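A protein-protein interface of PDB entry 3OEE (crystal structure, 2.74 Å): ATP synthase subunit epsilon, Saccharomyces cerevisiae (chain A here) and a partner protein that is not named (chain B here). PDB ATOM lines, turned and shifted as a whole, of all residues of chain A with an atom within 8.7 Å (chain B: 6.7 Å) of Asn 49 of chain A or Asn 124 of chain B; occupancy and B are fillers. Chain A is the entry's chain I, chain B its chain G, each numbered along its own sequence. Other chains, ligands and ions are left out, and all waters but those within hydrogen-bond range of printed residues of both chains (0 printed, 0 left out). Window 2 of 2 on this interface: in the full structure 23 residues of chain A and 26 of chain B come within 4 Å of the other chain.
N of Tyr 47 of chain A is in hydrogen-bond range of O of Lys 127 of chain B (2.5 Å).
The backbone carbonyl oxygen (O) of Tyr 47 of chain A sits close to the backbone carbonyl oxygen (O) of Ile 126 of chain B (2.8 Å).
The backbone carbonyl oxygen (O) of Asn 49 of chain A lies close to the backbone carbonyl oxygen (O) of Pro 123 of chain B (3.0 Å).
OD1 of Asn 124 of chain B sits close to O of Asn 49 of chain A.
The backbone NH of Lys 127 of chain B is in hydrogen-bond range of the backbone carbonyl oxygen of Ile 107 of chain B (2.9 Å).
N of Glu 55 of chain A lies close to O of Gln 46 of chain A, at 3.4 Å.
Among the printed residues, merely in contact across the chains: Gln 46 of chain A with Lys 127 of chain B (3.2 Å), Tyr 47 of chain A with Leu 119 of chain B (3.7 Å) and Ala 53 of chain A with Pro 123 of chain B (3.8 Å).
Of chain B, only Pro 123 (3.0 Å) and Asn 124 (3.4 Å) come within 4 Å of Asn 49 of chain A.
Of chain A, only Asn 49 (3.4 Å) comes within 4 Å of Asn 124 of chain B.
Printed residues of chain A within 4 Å of Lys 127 of chain B: Gln 46 (3.2 Å) and Tyr 47 (2.5 Å).
Printed residues of chain A within 4 Å of Ile 126 of chain B: Tyr 47.
Glu 55 of chain A touches none of the printed residues of chain B.
Asp 106 of chain B touches none of the printed residues of chain A.
Of the 11 printed residues of chain B, 5 touch a printed residue of chain A.
Hydrophobic or aromatic side chains of chain B within 4 Å of the printed part of chain A: Leu 119 and Pro 123.
Along chain B the printed residues that touch a printed residue of chain A span positions 119 to 127.
Of the 7 printed residues of chain A, 4 touch a printed residue of chain B.
Hydrophobic or aromatic side chains of chain A that line the printed part of chain B: Tyr 47.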
ATOM      1  N   GLN A  46      -3.297  -6.088  33.930  1.00  0.00           N
ATOM      2  CA  GLN A  46      -2.797  -7.435  33.741  1.00  0.00           C
ATOM      3  C   GLN A  46      -2.942  -7.767  32.266  1.00  0.00           C
ATOM      4  O   GLN A  46      -4.004  -7.554  31.684  1.00  0.00           O
ATOM      5  CB  GLN A  46      -3.578  -8.422  34.601  1.00  0.00           C
ATOM      6  CG  GLN A  46      -2.865  -9.749  34.822  1.00  0.00           C
ATOM      7  CD  GLN A  46      -3.523 -10.594  35.889  1.00  0.00           C
ATOM      8  OE1 GLN A  46      -4.138 -10.071  36.819  1.00  0.00           O
ATOM      9  NE2 GLN A  46      -3.394 -11.910  35.764  1.00  0.00           N
ATOM     10  N   TYR A  47      -1.863  -8.263  31.666  1.00  0.00           N
ATOM     11  CA  TYR A  47      -1.786  -8.460  30.214  1.00  0.00           C
ATOM     12  C   TYR A  47      -1.667  -9.929  29.831  1.00  0.00           C
ATOM     13  O   TYR A  47      -0.633 -10.556  30.062  1.00  0.00           O
ATOM     14  CB  TYR A  47      -0.606  -7.667  29.634  1.00  0.00           C
ATOM     15  CG  TYR A  47      -0.992  -6.402  28.891  1.00  0.00           C
ATOM     16  CD1 TYR A  47      -1.950  -5.522  29.405  1.00  0.00           C
ATOM     17  CD2 TYR A  47      -0.384  -6.075  27.676  1.00  0.00           C
ATOM     18  CE1 TYR A  47      -2.302  -4.354  28.717  1.00  0.00           C
ATOM     19  CE2 TYR A  47      -0.728  -4.908  26.979  1.00  0.00           C
ATOM     20  CZ  TYR A  47      -1.689  -4.054  27.507  1.00  0.00           C
ATOM     21  OH  TYR A  47      -2.038  -2.904  26.831  1.00  0.00           O
ATOM     22  N   LYS A  48      -2.728 -10.471  29.234  1.00  0.00           N
ATOM     23  CA  LYS A  48      -2.774 -11.888  28.868  1.00  0.00           C
ATOM     24  C   LYS A  48      -2.525 -12.127  27.377  1.00  0.00           C
ATOM     25  O   LYS A  48      -2.906 -11.311  26.531  1.00  0.00           O
ATOM     26  CB  LYS A  48      -4.105 -12.514  29.293  1.00  0.00           C
ATOM     27  N   ASN A  49      -1.894 -13.263  27.081  1.00  0.00           N
ATOM     28  CA  ASN A  49      -1.574 -13.696  25.714  1.00  0.00           C
ATOM     29  C   ASN A  49      -0.608 -12.762  24.994  1.00  0.00           C
ATOM     30  O   ASN A  49       0.290 -12.190  25.611  1.00  0.00           O
ATOM     31  CB  ASN A  49      -2.846 -13.914  24.875  1.00  0.00           C
ATOM     32  N   ALA A  53      -0.348  -9.882  23.880  1.00  0.00           N
ATOM     33  CA  ALA A  53      -1.652  -9.214  23.854  1.00  0.00           C
ATOM     34  C   ALA A  53      -2.118  -8.768  25.250  1.00  0.00           C
ATOM     35  O   ALA A  53      -1.369  -8.872  26.223  1.00  0.00           O
ATOM     36  CB  ALA A  53      -2.699 -10.111  23.185  1.00  0.00           C
ATOM     37  N   SER A  54      -3.363  -8.301  25.345  1.00  0.00           N
ATOM     38  CA  SER A  54      -3.853  -7.611  26.540  1.00  0.00           C
ATOM     39  C   SER A  54      -4.897  -8.390  27.361  1.00  0.00           C
ATOM     40  O   SER A  54      -5.357  -9.457  26.936  1.00  0.00           O
ATOM     41  CB  SER A  54      -4.430  -6.260  26.123  1.00  0.00           C
ATOM     42  OG  SER A  54      -4.870  -5.535  27.252  1.00  0.00           O
ATOM     43  N   GLU A  55      -5.248  -7.852  28.538  1.00  0.00           N
ATOM     44  CA  GLU A  55      -6.352  -8.377  29.380  1.00  0.00           C
ATOM     45  C   GLU A  55      -7.059  -7.279  30.238  1.00  0.00           C
ATOM     46  O   GLU A  55      -7.081  -6.120  29.819  1.00  0.00           O
ATOM     47  CB  GLU A  55      -5.910  -9.606  30.192  1.00  0.00           C
ATOM     48  N   ALA B 105      10.559 -16.454  31.804  1.00  0.00           N
ATOM     49  CA  ALA B 105      10.532 -15.502  32.910  1.00  0.00           C
ATOM     50  C   ALA B 105       9.321 -14.587  32.774  1.00  0.00           C
ATOM     51  O   ALA B 105       9.168 -13.921  31.751  1.00  0.00           O
ATOM     52  CB  ALA B 105      11.815 -14.686  32.932  1.00  0.00           C
ATOM     53  N   ASP B 106       8.455 -14.569  33.788  1.00  0.00           N
ATOM     54  CA  ASP B 106       7.302 -13.661  33.803  1.00  0.00           C
ATOM     55  C   ASP B 106       7.747 -12.197  33.858  1.00  0.00           C
ATOM     56  O   ASP B 106       8.771 -11.881  34.466  1.00  0.00           O
ATOM     57  CB  ASP B 106       6.377 -13.970  34.978  1.00  0.00           C
ATOM     58  CG  ASP B 106       5.557 -15.218  34.756  1.00  0.00           C
ATOM     59  OD1 ASP B 106       6.037 -16.320  35.104  1.00  0.00           O
ATOM     60  OD2 ASP B 106       4.426 -15.089  34.239  1.00  0.00           O
ATOM     61  N   ILE B 107       6.985 -11.309  33.217  1.00  0.00           N
ATOM     62  CA  ILE B 107       7.398  -9.907  33.089  1.00  0.00           C
ATOM     63  C   ILE B 107       6.351  -8.886  33.515  1.00  0.00           C
ATOM     64  O   ILE B 107       5.194  -8.938  33.096  1.00  0.00           O
ATOM     65  CB  ILE B 107       7.914  -9.572  31.661  1.00  0.00           C
ATOM     66  CG1 ILE B 107       9.177 -10.383  31.346  1.00  0.00           C
ATOM     67  CG2 ILE B 107       8.197  -8.078  31.529  1.00  0.00           C
ATOM     68  CD1 ILE B 107       9.810 -10.092  29.996  1.00  0.00           C
ATOM     69  N   LEU B 118       8.929  -4.278  24.566  1.00  0.00           N
ATOM     70  CA  LEU B 118       8.876  -5.685  24.971  1.00  0.00           C
ATOM     71  C   LEU B 118       7.608  -6.425  24.523  1.00  0.00           C
ATOM     72  O   LEU B 118       7.593  -7.656  24.475  1.00  0.00           O
ATOM     73  CB  LEU B 118       9.112  -5.829  26.480  1.00  0.00           C
ATOM     74  CG  LEU B 118      10.537  -6.166  26.963  1.00  0.00           C
ATOM     75  CD1 LEU B 118      11.636  -5.296  26.347  1.00  0.00           C
ATOM     76  CD2 LEU B 118      10.618  -6.130  28.483  1.00  0.00           C
ATOM     77  N   LEU B 119       6.557  -5.677  24.187  1.00  0.00           N
ATOM     78  CA  LEU B 119       5.302  -6.253  23.700  1.00  0.00           C
ATOM     79  C   LEU B 119       5.481  -6.779  22.286  1.00  0.00           C
ATOM     80  O   LEU B 119       4.916  -7.810  21.925  1.00  0.00           O
ATOM     81  CB  LEU B 119       4.186  -5.205  23.725  1.00  0.00           C
ATOM     82  CG  LEU B 119       2.730  -5.665  23.632  1.00  0.00           C
ATOM     83  CD1 LEU B 119       2.204  -6.023  25.015  1.00  0.00           C
ATOM     84  CD2 LEU B 119       1.863  -4.584  22.986  1.00  0.00           C
ATOM     85  N   HIS B 122       8.313  -9.827  22.721  1.00  0.00           N
ATOM     86  CA  HIS B 122       7.752 -10.979  23.452  1.00  0.00           C
ATOM     87  C   HIS B 122       6.368 -10.644  24.024  1.00  0.00           C
ATOM     88  O   HIS B 122       6.270 -10.222  25.177  1.00  0.00           O
ATOM     89  CB  HIS B 122       8.649 -11.400  24.626  1.00  0.00           C
ATOM     90  CG  HIS B 122      10.087 -11.598  24.268  1.00  0.00           C
ATOM     91  ND1 HIS B 122      11.081 -10.743  24.690  1.00  0.00           N
ATOM     92  CD2 HIS B 122      10.703 -12.566  23.552  1.00  0.00           C
ATOM     93  CE1 HIS B 122      12.248 -11.167  24.237  1.00  0.00           C
ATOM     94  NE2 HIS B 122      12.046 -12.272  23.544  1.00  0.00           N
ATOM     95  N   PRO B 123       5.293 -10.833  23.235  1.00  0.00           N
ATOM     96  CA  PRO B 123       3.942 -10.508  23.738  1.00  0.00           C
ATOM     97  C   PRO B 123       3.523 -11.248  25.023  1.00  0.00           C
ATOM     98  O   PRO B 123       2.847 -10.670  25.877  1.00  0.00           O
ATOM     99  CB  PRO B 123       3.023 -10.910  22.574  1.00  0.00           C
ATOM    100  CG  PRO B 123       3.865 -11.784  21.678  1.00  0.00           C
ATOM    101  CD  PRO B 123       5.264 -11.286  21.835  1.00  0.00           C
ATOM    102  N   ASN B 124       3.940 -12.503  25.160  1.00  0.00           N
ATOM    103  CA  ASN B 124       3.411 -13.387  26.202  1.00  0.00           C
ATOM    104  C   ASN B 124       4.024 -13.259  27.592  1.00  0.00           C
ATOM    105  O   ASN B 124       3.351 -13.530  28.591  1.00  0.00           O
ATOM    106  CB  ASN B 124       3.476 -14.847  25.746  1.00  0.00           C
ATOM    107  CG  ASN B 124       2.464 -15.162  24.675  1.00  0.00           C
ATOM    108  OD1 ASN B 124       2.176 -14.330  23.808  1.00  0.00           O
ATOM    109  ND2 ASN B 124       1.916 -16.369  24.722  1.00  0.00           N
ATOM    110  N   ASN B 125       5.296 -12.870  27.655  1.00  0.00           N
ATOM    111  CA  ASN B 125       6.004 -12.773  28.933  1.00  0.00           C
ATOM    112  C   ASN B 125       5.424 -11.677  29.827  1.00  0.00           C
ATOM    113  O   ASN B 125       5.298 -11.855  31.038  1.00  0.00           O
ATOM    114  CB  ASN B 125       7.504 -12.573  28.705  1.00  0.00           C
ATOM    115  CG  ASN B 125       8.133 -13.708  27.904  1.00  0.00           C
ATOM    116  OD1 ASN B 125       7.445 -14.460  27.212  1.00  0.00           O
ATOM    117  ND2 ASN B 125       9.453 -13.825  27.988  1.00  0.00           N
ATOM    118  N   ILE B 126       5.060 -10.560  29.212  1.00  0.00           N
ATOM    119  CA  ILE B 126       4.354  -9.488  29.897  1.00  0.00           C
ATOM    120  C   ILE B 126       3.019 -10.001  30.441  1.00  0.00           C
ATOM    121  O   ILE B 126       2.099 -10.301  29.674  1.00  0.00           O
ATOM    122  CB  ILE B 126       4.117  -8.276  28.954  1.00  0.00           C
ATOM    123  CG1 ILE B 126       5.437  -7.822  28.335  1.00  0.00           C
ATOM    124  CG2 ILE B 126       3.441  -7.123  29.701  1.00  0.00           C
ATOM    125  CD1 ILE B 126       5.275  -6.925  27.156  1.00  0.00           C
ATOM    126  N   LYS B 127       2.938 -10.117  31.765  1.00  0.00           N
ATOM    127  CA  LYS B 127       1.685 -10.450  32.432  1.00  0.00           C
ATOM    128  C   LYS B 127       1.087  -9.212  33.099  1.00  0.00           C
ATOM    129  O   LYS B 127      -0.126  -9.122  33.285  1.00  0.00           O
ATOM    130  CB  LYS B 127       1.879 -11.585  33.443  1.00  0.00           C
ATOM    131  CG  LYS B 127       0.570 -12.136  34.007  1.00  0.00           C
ATOM    132  CD  LYS B 127       0.784 -13.374  34.854  1.00  0.00           C
ATOM    133  CE  LYS B 127      -0.415 -13.620  35.754  1.00  0.00           C
ATOM    134  NZ  LYS B 127      -0.504 -15.035  36.193  1.00  0.00           N
